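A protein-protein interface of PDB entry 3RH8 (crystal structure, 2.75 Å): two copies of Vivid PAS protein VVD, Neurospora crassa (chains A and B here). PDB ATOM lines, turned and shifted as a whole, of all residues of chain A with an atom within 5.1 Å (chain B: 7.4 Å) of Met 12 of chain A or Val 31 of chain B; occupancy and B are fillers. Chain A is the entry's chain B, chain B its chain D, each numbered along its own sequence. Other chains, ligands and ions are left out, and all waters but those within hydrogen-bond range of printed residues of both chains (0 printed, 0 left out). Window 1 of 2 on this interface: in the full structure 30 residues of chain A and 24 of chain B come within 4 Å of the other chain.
The backbone carbonyl oxygen (O) of Ile 16 of chain B sits at hydrogen-bond distance from the side-chain amide nitrogen (ND2) of Asn 20 of chain B, at 3.3 Å.
The backbone NH (N) of Met 12 of chain A lies close to the side-chain carboxylate (OD1) of Asp 10 of chain A, at 3.5 Å.
The backbone NH (N) of Ser 34 of chain B sits at hydrogen-bond distance from the side-chain carboxylate (OD1) of Asp 32 of chain B.
The side-chain carboxylate (OD1) of Asp 10 of chain A sits at hydrogen-bond distance from the backbone NH (N) of Gly 13 of chain A.
The backbone NH (N) of Met 12 of chain A lies within hydrogen-bond range of the backbone carbonyl oxygen (O) of Val 31 of chain B (2.8 Å).
The backbone NH (N) of Ile 11 of chain A sits at hydrogen-bond distance from the backbone carbonyl oxygen (O) of Val 31 of chain B, 3.2 Å away.
The backbone carbonyl oxygen (O) of Tyr 4 of chain A lies within hydrogen-bond range of the backbone NH (N) of Asp 32 of chain B, at 2.9 Å.
The backbone NH (N) of Ala 5 of chain A sits close to the backbone carbonyl oxygen (O) of Pro 30 of chain B, at 3.3 Å.
The backbone NH of Val 31 of chain B is in hydrogen-bond range of the side-chain carboxylate of Asp 10 of chain A (3.1 Å).
The side-chain hydroxyl of Tyr 4 of chain A sits at hydrogen-bond distance from the backbone carbonyl oxygen of Phe 145 of chain B.
Met 12 of chain A touches Leu 15 of chain B, but with the chains exchanged Leu 15 of chain A does not touch Met 12 of chain B (4.1 Å).
Ile 16 of chain A touches Met 12 of chain B, but with the chains exchanged Met 12 of chain A does not touch Ile 16 of chain B (4.6 Å).
Ile 16 of chain A touches Leu 15 of chain B, but with the chains exchanged Leu 15 of chain A does not touch Ile 16 of chain B (6.0 Å).
Ile 16 of chain B touches its own counterpart, Ile 16 of chain A.
Positions printed for both chains: 11, 12, 14, 15 and 16.
Of chain B, only Leu 15 (3.0 Å) and Val 31 (2.8 Å) come within 4 Å of Met 12 of chain A.
Val 31 of chain B touches just these residues of chain A: Tyr 4, Ala 5, Asp 10, Ile 11 and Met 12.
Printed residues of chain B within 4 Å of Tyr 9 of chain A: Asp 32.
Printed residues of chain A within 4 Å of Ile 16 of chain B: Ile 16.
Of the printed residues of chain B, Ile 11 of chain A touches Val 31 (3.2 Å) and Asp 32 (3.96 Å).
Of the printed residues of chain A, Cys 35 of chain B touches Tyr 4 (3.3 Å).
The nearest residue of chain B that does not touch Met 12 of chain A is Met 19 of chain B (4.3 Å).
The nearest printed residue of chain A that does not touch Ile 16 of chain B is Met 12 of chain A (4.6 Å).
CD2 of Tyr 4 of chain A touches O of Leu 28 of chain B (3.4 Å).
Pro 30 of chain B touches Tyr 4 of chain A (O to C, 3.2 Å).
O of Tyr 4 of chain A touches CA of Val 31 of chain B (3.2 Å).
Cys 35 of chain B touches Tyr 4 of chain A (SG to CD1, 3.3 Å).
Ala 5 of chain A touches Val 31 of chain B (CB to N, 3.7 Å).
Ala 5 of chain A touches Asp 32 of chain B.
Asp 10 of chain A touches Pro 30 of chain B (CB to CB, 3.6 Å).
CG1 of Ile 16 of chain A touches CE of Met 12 of chain B, 3.8 Å away.
Ile 16 of chain A touches Leu 15 of chain B (CD1 to O, 3.9 Å).
CG2 of Ile 16 of chain A touches CG2 of Ile 16 of chain B (3.9 Å).
Hydrophobic or aromatic side chains of chain A within 4 Å of the printed part of chain B: Tyr 4, Ala 5, Ile 11, Met 12 and Ile 16.
Along chain A the printed residues that touch a printed residue of chain B span positions 4 to 16.
Among the printed residues, no Asp or Glu carboxylate lies within 4 Å of a Lys or Arg side-chain nitrogen of the other chain.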
ATOM      1  N   TYR A   4     -10.025  32.419  28.677  1.00  0.00           N
ATOM      2  CA  TYR A   4     -10.968  32.107  27.609  1.00  0.00           C
ATOM      3  C   TYR A   4     -12.397  32.553  27.886  1.00  0.00           C
ATOM      4  O   TYR A   4     -13.310  32.203  27.138  1.00  0.00           O
ATOM      5  CB  TYR A   4     -10.977  30.606  27.324  1.00  0.00           C
ATOM      6  CG  TYR A   4      -9.672  30.045  26.817  1.00  0.00           C
ATOM      7  CD1 TYR A   4      -9.026  30.609  25.717  1.00  0.00           C
ATOM      8  CD2 TYR A   4      -9.093  28.927  27.422  1.00  0.00           C
ATOM      9  CE1 TYR A   4      -7.837  30.078  25.226  1.00  0.00           C
ATOM     10  CE2 TYR A   4      -7.902  28.381  26.938  1.00  0.00           C
ATOM     11  CZ  TYR A   4      -7.278  28.962  25.839  1.00  0.00           C
ATOM     12  OH  TYR A   4      -6.110  28.420  25.360  1.00  0.00           O
ATOM     13  N   ALA A   5     -12.603  33.306  28.963  1.00  0.00           N
ATOM     14  CA  ALA A   5     -13.934  33.812  29.308  1.00  0.00           C
ATOM     15  C   ALA A   5     -13.834  35.234  29.856  1.00  0.00           C
ATOM     16  O   ALA A   5     -14.260  35.512  30.987  1.00  0.00           O
ATOM     17  CB  ALA A   5     -14.604  32.906  30.333  1.00  0.00           C
ATOM     18  N   TYR A   9     -18.267  34.838  32.263  1.00  0.00           N
ATOM     19  CA  TYR A   9     -19.097  33.664  32.468  1.00  0.00           C
ATOM     20  C   TYR A   9     -18.716  32.487  31.579  1.00  0.00           C
ATOM     21  O   TYR A   9     -18.389  32.655  30.413  1.00  0.00           O
ATOM     22  CB  TYR A   9     -20.570  34.025  32.231  1.00  0.00           C
ATOM     23  CG  TYR A   9     -21.099  35.061  33.194  1.00  0.00           C
ATOM     24  CD1 TYR A   9     -20.718  36.402  33.097  1.00  0.00           C
ATOM     25  CD2 TYR A   9     -21.957  34.699  34.227  1.00  0.00           C
ATOM     26  CE1 TYR A   9     -21.179  37.355  34.013  1.00  0.00           C
ATOM     27  CE2 TYR A   9     -22.419  35.642  35.140  1.00  0.00           C
ATOM     28  CZ  TYR A   9     -22.030  36.964  35.032  1.00  0.00           C
ATOM     29  OH  TYR A   9     -22.494  37.885  35.949  1.00  0.00           O
ATOM     30  N   ASP A  10     -18.760  31.289  32.146  1.00  0.00           N
ATOM     31  CA  ASP A  10     -18.445  30.095  31.385  1.00  0.00           C
ATOM     32  C   ASP A  10     -19.652  29.736  30.534  1.00  0.00           C
ATOM     33  O   ASP A  10     -20.387  28.798  30.852  1.00  0.00           O
ATOM     34  CB  ASP A  10     -18.103  28.931  32.321  1.00  0.00           C
ATOM     35  CG  ASP A  10     -17.839  27.607  31.572  1.00  0.00           C
ATOM     36  OD1 ASP A  10     -17.590  27.634  30.333  1.00  0.00           O
ATOM     37  OD2 ASP A  10     -17.866  26.537  32.240  1.00  0.00           O
ATOM     38  N   ILE A  11     -19.855  30.495  29.458  1.00  0.00           N
ATOM     39  CA  ILE A  11     -20.968  30.258  28.550  1.00  0.00           C
ATOM     40  C   ILE A  11     -20.941  28.847  27.954  1.00  0.00           C
ATOM     41  O   ILE A  11     -21.992  28.255  27.725  1.00  0.00           O
ATOM     42  CB  ILE A  11     -20.985  31.289  27.402  1.00  0.00           C
ATOM     43  CG1 ILE A  11     -21.292  32.680  27.957  1.00  0.00           C
ATOM     44  CG2 ILE A  11     -22.024  30.906  26.365  1.00  0.00           C
ATOM     45  CD1 ILE A  11     -22.581  32.760  28.768  1.00  0.00           C
ATOM     46  N   MET A  12     -19.751  28.311  27.698  1.00  0.00           N
ATOM     47  CA  MET A  12     -19.629  26.961  27.149  1.00  0.00           C
ATOM     48  C   MET A  12     -20.264  25.986  28.128  1.00  0.00           C
ATOM     49  O   MET A  12     -21.000  25.079  27.738  1.00  0.00           O
ATOM     50  CB  MET A  12     -18.148  26.589  26.949  1.00  0.00           C
ATOM     51  CG  MET A  12     -17.882  25.104  26.627  1.00  0.00           C
ATOM     52  SD  MET A  12     -16.230  24.570  27.199  1.00  0.00           S
ATOM     53  CE  MET A  12     -16.049  22.978  26.388  1.00  0.00           C
ATOM     54  N   GLY A  13     -19.972  26.192  29.408  1.00  0.00           N
ATOM     55  CA  GLY A  13     -20.505  25.333  30.449  1.00  0.00           C
ATOM     56  C   GLY A  13     -22.014  25.354  30.604  1.00  0.00           C
ATOM     57  O   GLY A  13     -22.638  24.315  30.793  1.00  0.00           O
ATOM     58  N   TYR A  14     -22.620  26.528  30.535  1.00  0.00           N
ATOM     59  CA  TYR A  14     -24.067  26.584  30.681  1.00  0.00           C
ATOM     60  C   TYR A  14     -24.776  25.964  29.479  1.00  0.00           C
ATOM     61  O   TYR A  14     -25.853  25.381  29.628  1.00  0.00           O
ATOM     62  CB  TYR A  14     -24.528  28.032  30.907  1.00  0.00           C
ATOM     63  CG  TYR A  14     -23.863  28.661  32.113  1.00  0.00           C
ATOM     64  CD1 TYR A  14     -23.811  27.982  33.326  1.00  0.00           C
ATOM     65  CD2 TYR A  14     -23.274  29.923  32.040  1.00  0.00           C
ATOM     66  CE1 TYR A  14     -23.191  28.536  34.435  1.00  0.00           C
ATOM     67  CE2 TYR A  14     -22.648  30.490  33.149  1.00  0.00           C
ATOM     68  CZ  TYR A  14     -22.612  29.788  34.343  1.00  0.00           C
ATOM     69  OH  TYR A  14     -21.996  30.327  35.453  1.00  0.00           O
ATOM     70  N   LEU A  15     -24.167  26.085  28.296  1.00  0.00           N
ATOM     71  CA  LEU A  15     -24.726  25.513  27.065  1.00  0.00           C
ATOM     72  C   LEU A  15     -24.681  23.994  27.152  1.00  0.00           C
ATOM     73  O   LEU A  15     -25.609  23.315  26.716  1.00  0.00           O
ATOM     74  CB  LEU A  15     -23.943  25.980  25.828  1.00  0.00           C
ATOM     75  CG  LEU A  15     -24.290  27.348  25.231  1.00  0.00           C
ATOM     76  CD1 LEU A  15     -23.465  27.586  23.984  1.00  0.00           C
ATOM     77  CD2 LEU A  15     -25.779  27.403  24.889  1.00  0.00           C
ATOM     78  N   ILE A  16     -23.592  23.468  27.714  1.00  0.00           N
ATOM     79  CA  ILE A  16     -23.441  22.026  27.894  1.00  0.00           C
ATOM     80  C   ILE A  16     -24.530  21.556  28.851  1.00  0.00           C
ATOM     81  O   ILE A  16     -25.190  20.556  28.589  1.00  0.00           O
ATOM     82  CB  ILE A  16     -22.061  21.661  28.494  1.00  0.00           C
ATOM     83  CG1 ILE A  16     -20.947  22.051  27.522  1.00  0.00           C
ATOM     84  CG2 ILE A  16     -22.002  20.172  28.818  1.00  0.00           C
ATOM     85  CD1 ILE A  16     -19.563  21.894  28.101  1.00  0.00           C
ATOM     86  N   ILE B  11     -19.271  20.722  16.820  1.00  0.00           N
ATOM     87  CA  ILE B  11     -18.392  21.425  17.739  1.00  0.00           C
ATOM     88  C   ILE B  11     -18.963  21.407  19.144  1.00  0.00           C
ATOM     89  O   ILE B  11     -18.251  21.126  20.102  1.00  0.00           O
ATOM     90  CB  ILE B  11     -18.188  22.895  17.308  1.00  0.00           C
ATOM     91  CG1 ILE B  11     -17.422  22.949  15.991  1.00  0.00           C
ATOM     92  CG2 ILE B  11     -17.437  23.659  18.387  1.00  0.00           C
ATOM     93  CD1 ILE B  11     -16.084  22.239  16.031  1.00  0.00           C
ATOM     94  N   MET B  12     -20.248  21.709  19.274  1.00  0.00           N
ATOM     95  CA  MET B  12     -20.844  21.712  20.589  1.00  0.00           C
ATOM     96  C   MET B  12     -20.625  20.347  21.219  1.00  0.00           C
ATOM     97  O   MET B  12     -20.337  20.244  22.408  1.00  0.00           O
ATOM     98  CB  MET B  12     -22.334  22.028  20.510  1.00  0.00           C
ATOM     99  CG  MET B  12     -22.939  22.441  21.859  1.00  0.00           C
ATOM    100  SD  MET B  12     -22.142  23.917  22.620  1.00  0.00           S
ATOM    101  CE  MET B  12     -21.092  23.120  23.844  1.00  0.00           C
ATOM    102  N   TYR B  14     -18.134  18.166  20.812  1.00  0.00           N
ATOM    103  CA  TYR B  14     -16.772  17.897  21.246  1.00  0.00           C
ATOM    104  C   TYR B  14     -16.451  18.708  22.492  1.00  0.00           C
ATOM    105  O   TYR B  14     -15.731  18.241  23.370  1.00  0.00           O
ATOM    106  CB  TYR B  14     -15.788  18.195  20.105  1.00  0.00           C
ATOM    107  CG  TYR B  14     -16.069  17.344  18.880  1.00  0.00           C
ATOM    108  CD1 TYR B  14     -16.037  15.949  18.956  1.00  0.00           C
ATOM    109  CD2 TYR B  14     -16.438  17.927  17.669  1.00  0.00           C
ATOM    110  CE1 TYR B  14     -16.372  15.156  17.861  1.00  0.00           C
ATOM    111  CE2 TYR B  14     -16.774  17.142  16.564  1.00  0.00           C
ATOM    112  CZ  TYR B  14     -16.741  15.759  16.670  1.00  0.00           C
ATOM    113  OH  TYR B  14     -17.098  14.985  15.590  1.00  0.00           O
ATOM    114  N   LEU B  15     -17.004  19.915  22.575  1.00  0.00           N
ATOM    115  CA  LEU B  15     -16.802  20.775  23.740  1.00  0.00           C
ATOM    116  C   LEU B  15     -17.378  20.070  24.962  1.00  0.00           C
ATOM    117  O   LEU B  15     -16.810  20.136  26.048  1.00  0.00           O
ATOM    118  CB  LEU B  15     -17.501  22.121  23.546  1.00  0.00           C
ATOM    119  CG  LEU B  15     -16.935  23.058  22.481  1.00  0.00           C
ATOM    120  CD1 LEU B  15     -17.765  24.326  22.436  1.00  0.00           C
ATOM    121  CD2 LEU B  15     -15.491  23.393  22.800  1.00  0.00           C
ATOM    122  N   ILE B  16     -18.517  19.406  24.776  1.00  0.00           N
ATOM    123  CA  ILE B  16     -19.158  18.651  25.854  1.00  0.00           C
ATOM    124  C   ILE B  16     -18.232  17.491  26.241  1.00  0.00           C
ATOM    125  O   ILE B  16     -17.799  17.366  27.390  1.00  0.00           O
ATOM    126  CB  ILE B  16     -20.484  18.025  25.402  1.00  0.00           C
ATOM    127  CG1 ILE B  16     -21.475  19.108  24.978  1.00  0.00           C
ATOM    128  CG2 ILE B  16     -21.039  17.161  26.523  1.00  0.00           C
ATOM    129  CD1 ILE B  16     -22.757  18.546  24.407  1.00  0.00           C
ATOM    130  N   GLN B  17     -17.938  16.644  25.258  1.00  0.00           N
ATOM    131  CA  GLN B  17     -17.072  15.500  25.470  1.00  0.00           C
ATOM    132  C   GLN B  17     -15.778  15.918  26.163  1.00  0.00           C
ATOM    133  O   GLN B  17     -15.286  15.217  27.050  1.00  0.00           O
ATOM    134  CB  GLN B  17     -16.743  14.831  24.135  1.00  0.00           C
ATOM    135  CG  GLN B  17     -16.381  13.361  24.293  1.00  0.00           C
ATOM    136  CD  GLN B  17     -15.857  12.720  23.022  1.00  0.00           C
ATOM    137  OE1 GLN B  17     -16.442  12.864  21.937  1.00  0.00           O
ATOM    138  NE2 GLN B  17     -14.751  11.988  23.152  1.00  0.00           N
ATOM    139  N   ILE B  18     -15.239  17.066  25.763  1.00  0.00           N
ATOM    140  CA  ILE B  18     -13.996  17.568  26.337  1.00  0.00           C
ATOM    141  C   ILE B  18     -14.100  17.976  27.803  1.00  0.00           C
ATOM    142  O   ILE B  18     -13.266  17.571  28.607  1.00  0.00           O
ATOM    143  CB  ILE B  18     -13.449  18.769  25.529  1.00  0.00           C
ATOM    144  CG1 ILE B  18     -12.978  18.293  24.150  1.00  0.00           C
ATOM    145  CG2 ILE B  18     -12.313  19.443  26.294  1.00  0.00           C
ATOM    146  CD1 ILE B  18     -12.561  19.408  23.228  1.00  0.00           C
ATOM    147  N   MET B  19     -15.109  18.776  28.153  1.00  0.00           N
ATOM    148  CA  MET B  19     -15.257  19.216  29.536  1.00  0.00           C
ATOM    149  C   MET B  19     -15.477  18.043  30.480  1.00  0.00           C
ATOM    150  O   MET B  19     -15.058  18.076  31.639  1.00  0.00           O
ATOM    151  CB  MET B  19     -16.408  20.213  29.696  1.00  0.00           C
ATOM    152  CG  MET B  19     -16.659  20.563  31.176  1.00  0.00           C
ATOM    153  SD  MET B  19     -17.802  21.928  31.570  1.00  0.00           S
ATOM    154  CE  MET B  19     -16.661  23.201  32.131  1.00  0.00           C
ATOM    155  N   ASN B  20     -16.126  16.997  29.987  1.00  0.00           N
ATOM    156  CA  ASN B  20     -16.380  15.833  30.821  1.00  0.00           C
ATOM    157  C   ASN B  20     -15.261  14.792  30.803  1.00  0.00           C
ATOM    158  O   ASN B  20     -15.417  13.691  31.337  1.00  0.00           O
ATOM    159  CB  ASN B  20     -17.714  15.200  30.434  1.00  0.00           C
ATOM    160  CG  ASN B  20     -18.888  16.062  30.846  1.00  0.00           C
ATOM    161  OD1 ASN B  20     -19.053  16.371  32.026  1.00  0.00           O
ATOM    162  ND2 ASN B  20     -19.704  16.465  29.878  1.00  0.00           N
ATOM    163  N   LEU B  28      -8.503  24.538  31.356  1.00  0.00           N
ATOM    164  CA  LEU B  28      -9.169  25.367  30.356  1.00  0.00           C
ATOM    165  C   LEU B  28      -9.863  26.564  30.993  1.00  0.00           C
ATOM    166  O   LEU B  28      -9.942  27.641  30.399  1.00  0.00           O
ATOM    167  CB  LEU B  28     -10.219  24.542  29.632  1.00  0.00           C
ATOM    168  CG  LEU B  28      -9.951  24.074  28.215  1.00  0.00           C
ATOM    169  CD1 LEU B  28     -11.123  23.219  27.762  1.00  0.00           C
ATOM    170  CD2 LEU B  28      -9.768  25.284  27.304  1.00  0.00           C
ATOM    171  N   GLY B  29     -10.377  26.353  32.202  1.00  0.00           N
ATOM    172  CA  GLY B  29     -11.093  27.394  32.912  1.00  0.00           C
ATOM    173  C   GLY B  29     -12.393  27.691  32.193  1.00  0.00           C
ATOM    174  O   GLY B  29     -12.834  26.892  31.368  1.00  0.00           O
ATOM    175  N   PRO B  30     -13.045  28.822  32.500  1.00  0.00           N
ATOM    176  CA  PRO B  30     -14.306  29.206  31.853  1.00  0.00           C
ATOM    177  C   PRO B  30     -14.101  29.626  30.384  1.00  0.00           C
ATOM    178  O   PRO B  30     -13.086  30.240  30.042  1.00  0.00           O
ATOM    179  CB  PRO B  30     -14.796  30.360  32.726  1.00  0.00           C
ATOM    180  CG  PRO B  30     -13.523  30.955  33.246  1.00  0.00           C
ATOM    181  CD  PRO B  30     -12.741  29.728  33.621  1.00  0.00           C
ATOM    182  N   VAL B  31     -15.066  29.303  29.524  1.00  0.00           N
ATOM    183  CA  VAL B  31     -14.971  29.641  28.106  1.00  0.00           C
ATOM    184  C   VAL B  31     -16.236  30.320  27.581  1.00  0.00           C
ATOM    185  O   VAL B  31     -17.321  29.752  27.666  1.00  0.00           O
ATOM    186  CB  VAL B  31     -14.694  28.359  27.257  1.00  0.00           C
ATOM    187  CG1 VAL B  31     -14.752  28.671  25.762  1.00  0.00           C
ATOM    188  CG2 VAL B  31     -13.337  27.789  27.619  1.00  0.00           C
ATOM    189  N   ASP B  32     -16.097  31.531  27.039  1.00  0.00           N
ATOM    190  CA  ASP B  32     -17.251  32.241  26.485  1.00  0.00           C
ATOM    191  C   ASP B  32     -17.236  32.285  24.950  1.00  0.00           C
ATOM    192  O   ASP B  32     -16.469  31.572  24.301  1.00  0.00           O
ATOM    193  CB  ASP B  32     -17.387  33.670  27.073  1.00  0.00           C
ATOM    194  CG  ASP B  32     -16.187  34.560  26.791  1.00  0.00           C
ATOM    195  OD1 ASP B  32     -15.634  34.484  25.673  1.00  0.00           O
ATOM    196  OD2 ASP B  32     -15.809  35.357  27.685  1.00  0.00           O
ATOM    197  N   THR B  33     -18.088  33.118  24.369  1.00  0.00           N
ATOM    198  CA  THR B  33     -18.168  33.203  22.924  1.00  0.00           C
ATOM    199  C   THR B  33     -17.033  33.979  22.259  1.00  0.00           C
ATOM    200  O   THR B  33     -16.898  33.964  21.035  1.00  0.00           O
ATOM    201  CB  THR B  33     -19.507  33.811  22.487  1.00  0.00           C
ATOM    202  OG1 THR B  33     -19.577  35.183  22.899  1.00  0.00           O
ATOM    203  CG2 THR B  33     -20.656  33.032  23.092  1.00  0.00           C
ATOM    204  N   SER B  34     -16.216  34.657  23.054  1.00  0.00           N
ATOM    205  CA  SER B  34     -15.106  35.415  22.493  1.00  0.00           C
ATOM    206  C   SER B  34     -13.915  34.489  22.222  1.00  0.00           C
ATOM    207  O   SER B  34     -12.950  34.869  21.562  1.00  0.00           O
ATOM    208  CB  SER B  34     -14.695  36.547  23.452  1.00  0.00           C
ATOM    209  OG  SER B  34     -14.202  36.041  24.678  1.00  0.00           O
ATOM    210  N   CYS B  35     -14.001  33.264  22.725  1.00  0.00           N
ATOM    211  CA  CYS B  35     -12.933  32.287  22.560  1.00  0.00           C
ATOM    212  C   CYS B  35     -12.836  31.750  21.128  1.00  0.00           C
ATOM    213  O   CYS B  35     -13.756  31.093  20.629  1.00  0.00           O
ATOM    214  CB  CYS B  35     -13.148  31.129  23.546  1.00  0.00           C
ATOM    215  SG  CYS B  35     -11.691  30.135  23.904  1.00  0.00           S
ATOM    216  N   ALA B  36     -11.717  32.045  20.472  1.00  0.00           N
ATOM    217  CA  ALA B  36     -11.480  31.573  19.110  1.00  0.00           C
ATOM    218  C   ALA B  36     -11.265  30.059  19.164  1.00  0.00           C
ATOM    219  O   ALA B  36     -10.428  29.571  19.929  1.00  0.00           O
ATOM    220  CB  ALA B  36     -10.261  32.257  18.515  1.00  0.00           C
ATOM    221  N   LEU B  37     -12.031  29.332  18.352  1.00  0.00           N
ATOM    222  CA  LEU B  37     -11.972  27.873  18.312  1.00  0.00           C
ATOM    223  C   LEU B  37     -11.642  27.271  16.950  1.00  0.00           C
ATOM    224  O   LEU B  37     -12.021  27.810  15.909  1.00  0.00           O
ATOM    225  CB  LEU B  37     -13.319  27.277  18.757  1.00  0.00           C
ATOM    226  CG  LEU B  37     -13.811  27.416  20.201  1.00  0.00           C
ATOM    227  CD1 LEU B  37     -15.234  26.885  20.310  1.00  0.00           C
ATOM    228  CD2 LEU B  37     -12.872  26.667  21.140  1.00  0.00           C
ATOM    229  N   MET B 143      -9.148  19.690  19.649  1.00  0.00           N
ATOM    230  CA  MET B 143      -9.707  21.034  19.769  1.00  0.00           C
ATOM    231  C   MET B 143      -8.692  22.056  20.278  1.00  0.00           C
ATOM    232  O   MET B 143      -8.039  21.843  21.301  1.00  0.00           O
ATOM    233  CB  MET B 143     -10.918  21.002  20.705  1.00  0.00           C
ATOM    234  CG  MET B 143     -11.724  22.286  20.762  1.00  0.00           C
ATOM    235  SD  MET B 143     -13.006  22.341  19.501  1.00  0.00           S
ATOM    236  CE  MET B 143     -14.321  21.421  20.329  1.00  0.00           C
ATOM    237  N   PHE B 145      -7.970  25.961  21.579  1.00  0.00           N
ATOM    238  CA  PHE B 145      -8.529  27.184  22.177  1.00  0.00           C
ATOM    239  C   PHE B 145      -7.423  28.242  22.151  1.00  0.00           C
ATOM    240  O   PHE B 145      -6.380  28.088  22.796  1.00  0.00           O
ATOM    241  CB  PHE B 145      -8.950  26.936  23.637  1.00  0.00           C
ATOM    242  CG  PHE B 145      -9.923  25.804  23.818  1.00  0.00           C
ATOM    243  CD1 PHE B 145     -11.233  26.055  24.210  1.00  0.00           C
ATOM    244  CD2 PHE B 145      -9.531  24.484  23.595  1.00  0.00           C
ATOM    245  CE1 PHE B 145     -12.140  25.009  24.380  1.00  0.00           C
ATOM    246  CE2 PHE B 145     -10.422  23.432  23.759  1.00  0.00           C
ATOM    247  CZ  PHE B 145     -11.733  23.692  24.150  1.00  0.00           C
